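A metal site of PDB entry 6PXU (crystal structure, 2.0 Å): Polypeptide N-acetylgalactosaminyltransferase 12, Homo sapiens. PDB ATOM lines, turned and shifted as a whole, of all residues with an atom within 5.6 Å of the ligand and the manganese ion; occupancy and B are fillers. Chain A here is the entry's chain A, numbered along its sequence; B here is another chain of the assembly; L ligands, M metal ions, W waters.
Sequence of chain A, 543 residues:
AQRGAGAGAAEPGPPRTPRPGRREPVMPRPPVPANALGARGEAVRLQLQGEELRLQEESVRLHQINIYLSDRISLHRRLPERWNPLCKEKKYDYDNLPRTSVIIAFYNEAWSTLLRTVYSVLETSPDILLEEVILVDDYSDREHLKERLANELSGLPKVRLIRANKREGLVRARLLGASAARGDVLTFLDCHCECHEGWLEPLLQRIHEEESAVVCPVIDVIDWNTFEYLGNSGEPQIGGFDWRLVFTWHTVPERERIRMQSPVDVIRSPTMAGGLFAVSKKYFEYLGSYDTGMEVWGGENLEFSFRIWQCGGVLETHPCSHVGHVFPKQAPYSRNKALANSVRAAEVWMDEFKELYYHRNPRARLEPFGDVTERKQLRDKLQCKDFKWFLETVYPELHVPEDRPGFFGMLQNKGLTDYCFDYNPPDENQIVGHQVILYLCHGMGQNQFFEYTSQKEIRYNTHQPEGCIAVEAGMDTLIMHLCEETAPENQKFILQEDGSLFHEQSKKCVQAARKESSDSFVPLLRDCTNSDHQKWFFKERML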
ATOM      1  N   ILE A 104     -19.738  25.133  15.289  1.00  0.00           N
ATOM      2  CA  ILE A 104     -20.338  25.999  14.269  1.00  0.00           C
ATOM      3  C   ILE A 104     -21.061  25.096  13.274  1.00  0.00           C
ATOM      4  O   ILE A 104     -20.442  24.587  12.327  1.00  0.00           O
ATOM      5  CB  ILE A 104     -19.293  26.867  13.557  1.00  0.00           C
ATOM      6  CG1 ILE A 104     -18.531  27.734  14.565  1.00  0.00           C
ATOM      7  CG2 ILE A 104     -19.976  27.714  12.460  1.00  0.00           C
ATOM      8  CD1 ILE A 104     -17.349  28.496  13.971  1.00  0.00           C
ATOM      9  N   ALA A 105     -22.354  24.915  13.448  1.00  0.00           N
ATOM     10  CA  ALA A 105     -23.155  24.228  12.439  1.00  0.00           C
ATOM     11  C   ALA A 105     -23.491  25.213  11.308  1.00  0.00           C
ATOM     12  O   ALA A 105     -23.700  26.406  11.549  1.00  0.00           O
ATOM     13  CB  ALA A 105     -24.414  23.651  13.076  1.00  0.00           C
ATOM     14  N   PHE A 106     -23.470  24.731  10.073  1.00  0.00           N
ATOM     15  CA  PHE A 106     -23.731  25.598   8.944  1.00  0.00           C
ATOM     16  C   PHE A 106     -24.552  24.878   7.904  1.00  0.00           C
ATOM     17  O   PHE A 106     -24.423  23.654   7.704  1.00  0.00           O
ATOM     18  CB  PHE A 106     -22.427  26.168   8.304  1.00  0.00           C
ATOM     19  CG  PHE A 106     -21.546  25.147   7.624  1.00  0.00           C
ATOM     20  CD1 PHE A 106     -21.738  24.831   6.288  1.00  0.00           C
ATOM     21  CD2 PHE A 106     -20.498  24.553   8.296  1.00  0.00           C
ATOM     22  CE1 PHE A 106     -20.935  23.915   5.641  1.00  0.00           C
ATOM     23  CE2 PHE A 106     -19.660  23.649   7.647  1.00  0.00           C
ATOM     24  CZ  PHE A 106     -19.878  23.330   6.319  1.00  0.00           C
ATOM     25  N   TYR A 107     -25.451  25.634   7.269  1.00  0.00           N
ATOM     26  CA  TYR A 107     -26.308  25.121   6.203  1.00  0.00           C
ATOM     27  C   TYR A 107     -26.330  26.142   5.083  1.00  0.00           C
ATOM     28  O   TYR A 107     -26.971  27.193   5.216  1.00  0.00           O
ATOM     29  CB  TYR A 107     -27.723  24.840   6.715  1.00  0.00           C
ATOM     30  CG  TYR A 107     -28.652  24.468   5.579  1.00  0.00           C
ATOM     31  CD1 TYR A 107     -28.479  23.291   4.883  1.00  0.00           C
ATOM     32  CD2 TYR A 107     -29.676  25.325   5.194  1.00  0.00           C
ATOM     33  CE1 TYR A 107     -29.297  22.972   3.832  1.00  0.00           C
ATOM     34  CE2 TYR A 107     -30.514  25.011   4.149  1.00  0.00           C
ATOM     35  CZ  TYR A 107     -30.314  23.832   3.465  1.00  0.00           C
ATOM     36  OH  TYR A 107     -31.124  23.486   2.426  1.00  0.00           O
ATOM     37  N   GLU A 109     -24.317  28.299   3.968  1.00  0.00           N
ATOM     38  CA  GLU A 109     -23.735  29.615   4.193  1.00  0.00           C
ATOM     39  C   GLU A 109     -22.817  29.989   3.024  1.00  0.00           C
ATOM     40  O   GLU A 109     -22.229  29.131   2.365  1.00  0.00           O
ATOM     41  CB  GLU A 109     -22.943  29.614   5.515  1.00  0.00           C
ATOM     42  CG  GLU A 109     -22.431  30.987   5.977  1.00  0.00           C
ATOM     43  CD  GLU A 109     -23.565  31.985   6.233  1.00  0.00           C
ATOM     44  OE1 GLU A 109     -24.667  31.552   6.653  1.00  0.00           O
ATOM     45  OE2 GLU A 109     -23.365  33.204   6.000  1.00  0.00           O
ATOM     46  N   VAL A 136     -19.796  21.810  11.526  1.00  0.00           N
ATOM     47  CA  VAL A 136     -20.743  20.746  11.206  1.00  0.00           C
ATOM     48  C   VAL A 136     -21.534  21.179   9.986  1.00  0.00           C
ATOM     49  O   VAL A 136     -22.378  22.072  10.057  1.00  0.00           O
ATOM     50  CB  VAL A 136     -21.691  20.432  12.376  1.00  0.00           C
ATOM     51  CG1 VAL A 136     -22.509  19.193  12.038  1.00  0.00           C
ATOM     52  CG2 VAL A 136     -20.887  20.258  13.665  1.00  0.00           C
ATOM     53  N   ASP A 138     -24.456  20.768   7.855  1.00  0.00           N
ATOM     54  CA  ASP A 138     -25.785  20.172   7.946  1.00  0.00           C
ATOM     55  C   ASP A 138     -26.342  19.867   6.556  1.00  0.00           C
ATOM     56  O   ASP A 138     -27.413  20.322   6.163  1.00  0.00           O
ATOM     57  CB  ASP A 138     -26.735  21.091   8.735  1.00  0.00           C
ATOM     58  CG  ASP A 138     -28.099  20.450   8.949  1.00  0.00           C
ATOM     59  OD1 ASP A 138     -28.180  19.200   8.830  1.00  0.00           O
ATOM     60  OD2 ASP A 138     -29.072  21.197   9.249  1.00  0.00           O
ATOM     61  N   ARG A 167     -30.107  15.932   6.009  1.00  0.00           N
ATOM     62  CA  ARG A 167     -30.488  17.198   6.613  1.00  0.00           C
ATOM     63  C   ARG A 167     -30.899  16.962   8.066  1.00  0.00           C
ATOM     64  O   ARG A 167     -31.804  16.161   8.354  1.00  0.00           O
ATOM     65  CB  ARG A 167     -31.620  17.825   5.794  1.00  0.00           C
ATOM     66  CG  ARG A 167     -32.039  19.185   6.303  1.00  0.00           C
ATOM     67  CD  ARG A 167     -30.955  20.228   6.084  1.00  0.00           C
ATOM     68  NE  ARG A 167     -31.297  21.476   6.752  1.00  0.00           N
ATOM     69  CZ  ARG A 167     -32.157  22.358   6.258  1.00  0.00           C
ATOM     70  NH1 ARG A 167     -32.748  22.130   5.090  1.00  0.00           N
ATOM     71  NH2 ARG A 167     -32.428  23.467   6.931  1.00  0.00           N
ATOM     72  N   GLU A 168     -30.223  17.629   8.990  1.00  0.00           N
ATOM     73  CA  GLU A 168     -30.500  17.425  10.407  1.00  0.00           C
ATOM     74  C   GLU A 168     -31.276  18.560  11.038  1.00  0.00           C
ATOM     75  O   GLU A 168     -32.033  18.322  11.978  1.00  0.00           O
ATOM     76  CB  GLU A 168     -29.181  17.242  11.193  1.00  0.00           C
ATOM     77  CG  GLU A 168     -28.398  15.978  10.820  1.00  0.00           C
ATOM     78  CD  GLU A 168     -29.091  14.698  11.260  1.00  0.00           C
ATOM     79  OE1 GLU A 168     -30.084  14.754  12.016  1.00  0.00           O
ATOM     80  OE2 GLU A 168     -28.646  13.614  10.824  1.00  0.00           O
ATOM     81  N   GLY A 169     -31.117  19.781  10.554  1.00  0.00           N
ATOM     82  CA  GLY A 169     -31.598  20.935  11.289  1.00  0.00           C
ATOM     83  C   GLY A 169     -30.566  21.371  12.308  1.00  0.00           C
ATOM     84  O   GLY A 169     -29.669  20.615  12.690  1.00  0.00           O
ATOM     85  N   LEU A 170     -30.690  22.629  12.757  1.00  0.00           N
ATOM     86  CA  LEU A 170     -29.643  23.203  13.585  1.00  0.00           C
ATOM     87  C   LEU A 170     -29.511  22.490  14.926  1.00  0.00           C
ATOM     88  O   LEU A 170     -28.400  22.346  15.445  1.00  0.00           O
ATOM     89  CB  LEU A 170     -29.850  24.708  13.773  1.00  0.00           C
ATOM     90  CG  LEU A 170     -30.902  25.298  14.691  1.00  0.00           C
ATOM     91  CD1 LEU A 170     -30.368  25.471  16.095  1.00  0.00           C
ATOM     92  CD2 LEU A 170     -31.360  26.631  14.115  1.00  0.00           C
ATOM     93  N   ALA A 173     -27.718  19.066  14.201  1.00  0.00           N
ATOM     94  CA  ALA A 173     -26.373  19.362  13.731  1.00  0.00           C
ATOM     95  C   ALA A 173     -25.477  19.837  14.875  1.00  0.00           C
ATOM     96  O   ALA A 173     -24.307  19.425  14.976  1.00  0.00           O
ATOM     97  CB  ALA A 173     -26.415  20.407  12.604  1.00  0.00           C
ATOM     98  N   ARG A 174     -26.023  20.709  15.730  1.00  0.00           N
ATOM     99  CA  ARG A 174     -25.289  21.113  16.924  1.00  0.00           C
ATOM    100  C   ARG A 174     -24.971  19.926  17.812  1.00  0.00           C
ATOM    101  O   ARG A 174     -23.878  19.832  18.362  1.00  0.00           O
ATOM    102  CB  ARG A 174     -26.083  22.129  17.724  1.00  0.00           C
ATOM    103  CG  ARG A 174     -25.904  23.486  17.195  1.00  0.00           C
ATOM    104  CD  ARG A 174     -26.767  24.502  17.859  1.00  0.00           C
ATOM    105  NE  ARG A 174     -26.176  25.755  17.464  1.00  0.00           N
ATOM    106  CZ  ARG A 174     -26.732  26.945  17.542  1.00  0.00           C
ATOM    107  NH1 ARG A 174     -26.019  27.984  17.115  1.00  0.00           N
ATOM    108  NH2 ARG A 174     -27.973  27.081  17.996  1.00  0.00           N
ATOM    109  N   LEU A 189     -21.442  29.007  18.170  1.00  0.00           N
ATOM    110  CA  LEU A 189     -21.517  30.208  17.340  1.00  0.00           C
ATOM    111  C   LEU A 189     -22.257  29.874  16.044  1.00  0.00           C
ATOM    112  O   LEU A 189     -22.354  28.714  15.643  1.00  0.00           O
ATOM    113  CB  LEU A 189     -20.120  30.754  17.033  1.00  0.00           C
ATOM    114  CG  LEU A 189     -19.253  31.107  18.243  1.00  0.00           C
ATOM    115  CD1 LEU A 189     -17.903  31.566  17.740  1.00  0.00           C
ATOM    116  CD2 LEU A 189     -19.890  32.210  19.098  1.00  0.00           C
ATOM    117  N   ASP A 190     -22.819  30.913  15.402  1.00  0.00           N
ATOM    118  CA  ASP A 190     -23.353  30.773  14.057  1.00  0.00           C
ATOM    119  C   ASP A 190     -22.233  30.903  13.035  1.00  0.00           C
ATOM    120  O   ASP A 190     -21.137  31.392  13.329  1.00  0.00           O
ATOM    121  CB  ASP A 190     -24.431  31.839  13.789  1.00  0.00           C
ATOM    122  CG  ASP A 190     -25.722  31.582  14.543  1.00  0.00           C
ATOM    123  OD1 ASP A 190     -25.799  30.597  15.319  1.00  0.00           O
ATOM    124  OD2 ASP A 190     -26.663  32.384  14.381  1.00  0.00           O
ATOM    125  N   CYS A 191     -22.531  30.522  11.805  1.00  0.00           N
ATOM    126  CA  CYS A 191     -21.519  30.540  10.758  1.00  0.00           C
ATOM    127  C   CYS A 191     -21.386  31.908  10.094  1.00  0.00           C
ATOM    128  O   CYS A 191     -20.803  31.999   9.006  1.00  0.00           O
ATOM    129  CB  CYS A 191     -21.842  29.466   9.721  1.00  0.00           C
ATOM    130  SG  CYS A 191     -23.475  29.727   8.994  1.00  0.00           S
ATOM    131  N   HIS A 192     -21.909  32.974  10.716  1.00  0.00           N
ATOM    132  CA  HIS A 192     -21.762  34.325  10.177  1.00  0.00           C
ATOM    133  C   HIS A 192     -21.570  35.274  11.357  1.00  0.00           C
ATOM    134  O   HIS A 192     -22.346  36.191  11.593  1.00  0.00           O
ATOM    135  CB  HIS A 192     -22.985  34.713   9.333  1.00  0.00           C
ATOM    136  CG  HIS A 192     -24.253  34.139   9.857  1.00  0.00           C
ATOM    137  ND1 HIS A 192     -24.909  33.104   9.228  1.00  0.00           N
ATOM    138  CD2 HIS A 192     -24.926  34.376  11.005  1.00  0.00           C
ATOM    139  CE1 HIS A 192     -25.967  32.759   9.951  1.00  0.00           C
ATOM    140  NE2 HIS A 192     -26.004  33.527  11.027  1.00  0.00           N
ATOM    141  N   VAL A 296     -35.229  21.762  11.965  1.00  0.00           N
ATOM    142  CA  VAL A 296     -34.788  22.884  11.118  1.00  0.00           C
ATOM    143  C   VAL A 296     -34.359  24.127  11.909  1.00  0.00           C
ATOM    144  O   VAL A 296     -33.165  24.426  11.974  1.00  0.00           O
ATOM    145  CB  VAL A 296     -35.876  23.249  10.086  1.00  0.00           C
ATOM    146  CG1 VAL A 296     -35.360  24.370   9.172  1.00  0.00           C
ATOM    147  CG2 VAL A 296     -36.287  22.022   9.266  1.00  0.00           C
ATOM    148  N   TRP A 297     -35.319  24.868  12.470  1.00  0.00           N
ATOM    149  CA  TRP A 297     -35.046  26.210  13.013  1.00  0.00           C
ATOM    150  C   TRP A 297     -36.191  26.655  13.915  1.00  0.00           C
ATOM    151  O   TRP A 297     -37.352  26.297  13.678  1.00  0.00           O
ATOM    152  CB  TRP A 297     -34.855  27.251  11.907  1.00  0.00           C
ATOM    153  CG  TRP A 297     -34.608  28.672  12.406  1.00  0.00           C
ATOM    154  CD1 TRP A 297     -33.394  29.257  12.596  1.00  0.00           C
ATOM    155  CD2 TRP A 297     -35.598  29.675  12.710  1.00  0.00           C
ATOM    156  NE1 TRP A 297     -33.568  30.551  13.046  1.00  0.00           N
ATOM    157  CE2 TRP A 297     -34.904  30.836  13.120  1.00  0.00           C
ATOM    158  CE3 TRP A 297     -37.005  29.697  12.693  1.00  0.00           C
ATOM    159  CZ2 TRP A 297     -35.559  31.998  13.497  1.00  0.00           C
ATOM    160  CZ3 TRP A 297     -37.655  30.867  13.067  1.00  0.00           C
ATOM    161  CH2 TRP A 297     -36.935  31.996  13.473  1.00  0.00           C
ATOM    162  N   HIS A 325     -22.938  39.474  14.776  1.00  0.00           N
ATOM    163  CA  HIS A 325     -23.743  38.461  14.096  1.00  0.00           C
ATOM    164  C   HIS A 325     -24.403  39.108  12.880  1.00  0.00           C
ATOM    165  O   HIS A 325     -24.994  40.189  13.015  1.00  0.00           O
ATOM    166  CB  HIS A 325     -24.781  37.903  15.084  1.00  0.00           C
ATOM    167  CG  HIS A 325     -25.766  36.954  14.475  1.00  0.00           C
ATOM    168  ND1 HIS A 325     -26.926  37.376  13.851  1.00  0.00           N
ATOM    169  CD2 HIS A 325     -25.774  35.604  14.398  1.00  0.00           C
ATOM    170  CE1 HIS A 325     -27.606  36.338  13.420  1.00  0.00           C
ATOM    171  NE2 HIS A 325     -26.928  35.242  13.736  1.00  0.00           N
ATOM    172  N   VAL A 326     -24.269  38.505  11.709  1.00  0.00           N
ATOM    173  CA  VAL A 326     -24.888  39.082  10.521  1.00  0.00           C
ATOM    174  C   VAL A 326     -26.366  38.681  10.465  1.00  0.00           C
ATOM    175  O   VAL A 326     -26.716  37.667   9.862  1.00  0.00           O
ATOM    176  CB  VAL A 326     -24.200  38.662   9.212  1.00  0.00           C
ATOM    177  CG1 VAL A 326     -24.807  39.465   8.033  1.00  0.00           C
ATOM    178  CG2 VAL A 326     -22.732  38.892   9.304  1.00  0.00           C
ATOM    179  N   PRO A 328     -29.764  38.492   8.903  1.00  0.00           N
ATOM    180  CA  PRO A 328     -30.107  38.584   7.477  1.00  0.00           C
ATOM    181  C   PRO A 328     -31.271  39.528   7.199  1.00  0.00           C
ATOM    182  O   PRO A 328     -32.044  39.893   8.077  1.00  0.00           O
ATOM    183  CB  PRO A 328     -30.457  37.137   7.131  1.00  0.00           C
ATOM    184  CG  PRO A 328     -30.978  36.568   8.398  1.00  0.00           C
ATOM    185  CD  PRO A 328     -30.186  37.217   9.499  1.00  0.00           C
ATOM    186  N   PRO A 332     -33.151  33.202   5.278  1.00  0.00           N
ATOM    187  CA  PRO A 332     -32.443  32.750   4.061  1.00  0.00           C
ATOM    188  C   PRO A 332     -32.889  31.396   3.533  1.00  0.00           C
ATOM    189  O   PRO A 332     -32.488  31.018   2.417  1.00  0.00           O
ATOM    190  CB  PRO A 332     -30.966  32.694   4.516  1.00  0.00           C
ATOM    191  CG  PRO A 332     -30.930  33.220   5.917  1.00  0.00           C
ATOM    192  CD  PRO A 332     -32.310  33.099   6.482  1.00  0.00           C
ATOM    193  N   TYR A 333     -33.706  30.660   4.282  1.00  0.00           N
ATOM    194  CA  TYR A 333     -34.213  29.357   3.884  1.00  0.00           C
ATOM    195  C   TYR A 333     -35.580  29.225   4.551  1.00  0.00           C
ATOM    196  O   TYR A 333     -35.916  30.005   5.457  1.00  0.00           O
ATOM    197  CB  TYR A 333     -33.239  28.235   4.288  1.00  0.00           C
ATOM    198  CG  TYR A 333     -32.858  28.346   5.749  1.00  0.00           C
ATOM    199  CD1 TYR A 333     -33.709  27.840   6.754  1.00  0.00           C
ATOM    200  CD2 TYR A 333     -31.706  29.025   6.149  1.00  0.00           C
ATOM    201  CE1 TYR A 333     -33.408  27.980   8.100  1.00  0.00           C
ATOM    202  CE2 TYR A 333     -31.391  29.160   7.512  1.00  0.00           C
ATOM    203  CZ  TYR A 333     -32.247  28.628   8.469  1.00  0.00           C
ATOM    204  OH  TYR A 333     -31.970  28.771   9.811  1.00  0.00           O
ATOM    205  N   ARG A 335     -38.341  28.521   6.925  1.00  0.00           N
ATOM    206  CA  ARG A 335     -38.495  28.259   8.352  1.00  0.00           C
ATOM    207  C   ARG A 335     -39.976  27.997   8.607  1.00  0.00           C
ATOM    208  O   ARG A 335     -40.757  28.889   8.911  1.00  0.00           O
ATOM    209  CB  ARG A 335     -37.949  29.399   9.161  1.00  0.00           C
ATOM    210  CG  ARG A 335     -36.419  29.484   9.114  1.00  0.00           C
ATOM    211  CD  ARG A 335     -35.980  30.879   9.459  1.00  0.00           C
ATOM    212  NE  ARG A 335     -34.545  31.039   9.539  1.00  0.00           N
ATOM    213  CZ  ARG A 335     -33.940  32.178   9.854  1.00  0.00           C
ATOM    214  NH1 ARG A 335     -32.621  32.245   9.909  1.00  0.00           N
ATOM    215  NH2 ARG A 335     -34.674  33.254  10.119  1.00  0.00           N
ATOM    216  N   ILE B  13     -37.809  35.129  11.887  1.00  0.00           N
ATOM    217  CA  ILE B  13     -36.501  35.768  12.020  1.00  0.00           C
ATOM    218  C   ILE B  13     -36.188  35.984  13.500  1.00  0.00           C
ATOM    219  O   ILE B  13     -37.088  36.083  14.347  1.00  0.00           O
ATOM    220  CB  ILE B  13     -36.401  37.132  11.282  1.00  0.00           C
ATOM    221  CG1 ILE B  13     -37.589  38.036  11.631  1.00  0.00           C
ATOM    222  CG2 ILE B  13     -36.238  36.953   9.782  1.00  0.00           C
ATOM    223  CD1 ILE B  13     -37.604  39.344  10.863  1.00  0.00           C
ATOM    224  N   THR B  14     -34.893  36.068  13.804  1.00  0.00           N
ATOM    225  CA  THR B  14     -34.427  36.510  15.110  1.00  0.00           C
ATOM    226  C   THR B  14     -34.251  38.030  15.100  1.00  0.00           C
ATOM    227  O   THR B  14     -33.523  38.550  14.249  1.00  0.00           O
ATOM    228  CB  THR B  14     -33.118  35.839  15.475  1.00  0.00           C
ATOM    229  OG1 THR B  14     -33.356  34.451  15.731  1.00  0.00           O
ATOM    230  CG2 THR B  14     -32.495  36.466  16.718  1.00  0.00           C
HETATM  231  N1  LIG L   1     -28.386  25.942  10.520  1.00  0.00           N
HETATM  232  C1  LIG L   1     -28.137  24.594  10.318  1.00  0.00           C
HETATM  233  N2  LIG L   1     -29.128  23.783   9.831  1.00  0.00           N
HETATM  234  C2  LIG L   1     -30.369  24.335   9.555  1.00  0.00           C
HETATM  235  C3  LIG L   1     -30.610  25.692   9.763  1.00  0.00           C
HETATM  236  C4  LIG L   1     -29.594  26.521  10.240  1.00  0.00           C
HETATM  237  O1  LIG L   1     -27.027  24.122  10.595  1.00  0.00           O
HETATM  238  O2  LIG L   1     -31.230  23.592   9.123  1.00  0.00           O
HETATM  239  C5  LIG L   1     -27.261  26.708  11.075  1.00  0.00           C
HETATM  240  C6  LIG L   1     -27.034  28.072  10.445  1.00  0.00           C
HETATM  241  O3  LIG L   1     -26.029  27.964   9.459  1.00  0.00           O
HETATM  242  C7  LIG L   1     -26.555  28.853  11.651  1.00  0.00           C
HETATM  243  C8  LIG L   1     -27.342  28.225  12.799  1.00  0.00           C
HETATM  244  O4  LIG L   1     -27.470  26.893  12.463  1.00  0.00           O
HETATM  245  O5  LIG L   1     -25.139  28.656  11.804  1.00  0.00           O
HETATM  246  C9  LIG L   1     -28.811  28.622  12.743  1.00  0.00           C
HETATM  247  O6  LIG L   1     -28.781  29.983  12.642  1.00  0.00           O
HETATM  248  P1  LIG L   1     -29.425  30.949  11.527  1.00  0.00           P
HETATM  249  O7  LIG L   1     -29.872  30.493  10.185  1.00  0.00           O
HETATM  250  O8  LIG L   1     -28.358  31.979  11.454  1.00  0.00           O
HETATM  251  O9  LIG L   1     -30.674  31.530  12.350  1.00  0.00           O
HETATM  252  P2  LIG L   1     -30.770  33.044  12.894  1.00  0.00           P
HETATM  253  O10 LIG L   1     -31.952  33.067  13.789  1.00  0.00           O
HETATM  254  O11 LIG L   1     -30.929  33.953  11.726  1.00  0.00           O
HETATM  255  O12 LIG L   1     -29.563  33.424  13.674  1.00  0.00           O
HETATM  256 MN    MN M   1     -27.596  33.491  12.622  1.00  0.00          MN
HETATM  257  O   HOH W   1     -33.258  35.378  11.654  1.00  0.00           O
HETATM  258  O   HOH W   2     -28.599  31.101   7.730  1.00  0.00           O
HETATM  259  O   HOH W   3     -28.694  34.895  11.046  1.00  0.00           O
HETATM  260  O   HOH W   4     -26.239  29.571   7.319  1.00  0.00           O
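NH2 of Arg 167 lies within hydrogen-bond range of O2 of the ligand (2.5 Å).
OD2 of Asp 138 is in hydrogen-bond range of N2 of the ligand (2.7 Å).
The backbone carbonyl oxygen of Ala 105 is in hydrogen-bond range of an oxygen (O5) of the ligand.
The side-chain hydroxyl of Tyr 333 is in hydrogen-bond range of an oxygen (O7) of the ligand.
OG1 of Thr 14 of chain B sits at hydrogen-bond distance from O10 of the ligand (2.8 Å).
The guanidinium group of Arg 335 lies within salt-bridge range of an oxygen (O11) of the ligand (3.0 Å).
An oxygen (O10) of the ligand is in hydrogen-bond range of the indole nitrogen (NE1) of Trp 297 (3.1 Å).
O5 of the ligand lies within hydrogen-bond range of N of Cys 191.
An oxygen (O3) of the ligand lies within hydrogen-bond range of the side-chain sulfur (SG) of Cys 191 (3.1 Å).
O3 of the ligand lies within hydrogen-bond range of N of Tyr 107 (3.2 Å).
The side-chain sulfur of Cys 191 is in hydrogen-bond range of a ring nitrogen (ND1) of His 192, at 3.7 Å.
ND1 of His 192 is in hydrogen-bond range of OE1 of Glu 109 (3.0 Å).
OD1 of Asp 190 lies within salt-bridge range of NH1 of Arg 174 (3.2 Å).
OD2 of Asp 138 sits at hydrogen-bond distance from N of Gly 169 (2.8 Å).
N of Glu 168 lies within hydrogen-bond range of OD1 of Asp 138.
NE of Arg 335 lies within hydrogen-bond range of OH of Tyr 333 (3.4 Å).
N of Phe 106 is in hydrogen-bond range of O of Val 136, at 2.9 Å.
The backbone NH (N) of Leu 170 sits at hydrogen-bond distance from the backbone carbonyl oxygen (O) of Val 296 (3.2 Å).
The nearest printed residue that does not touch the manganese ion is Val 326 (5.1 Å).
Water W4 lies within hydrogen-bond range of the side-chain carboxylate of Glu 109 (2.6 Å), an oxygen (O3) of the ligand (2.7 Å), the side-chain sulfur of Cys 191 (3.2 Å) and the backbone carbonyl oxygen of Tyr 107 (3.3 Å).
Water W1 lies within hydrogen-bond range of O11 of the ligand (2.7 Å), N of Thr 14 of chain B (2.8 Å) and NH2 of Arg 335 (3.0 Å).
Residues that only touch the ligand: Phe 106 (3.3 Å), Gly 169 (3.4 Å), Leu 170 (3.5 Å) and Val 296 (3.5 Å).
Hydrophobic or aromatic side chains within 4 Å of the ligand: Ala 105, Tyr 107, Leu 170, His 192, Trp 297, His 325 and Tyr 333.
Within 4 Å of the ligand: Ala 105, Phe 106, Tyr 107, Asp 138, Arg 167, Gly 169, Leu 170, Asp 190, Cys 191, His 192, Val 296, Trp 297, His 325, Tyr 333, Arg 335 and Thr 14 of chain B.
The nearest printed residue that does not touch the ligand is Pro 328 (4.02 Å).
The manganese ion is bound by an oxygen (O8) of the ligand (2.1 Å), a ring nitrogen (NE2) of His 325 (2.2 Å), an oxygen (O12) of the ligand (2.2 Å), a ring nitrogen (NE2) of His 192 (2.3 Å), the side-chain carboxylate of Asp 190 (2.3 Å) and water W3 (2.4 Å).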
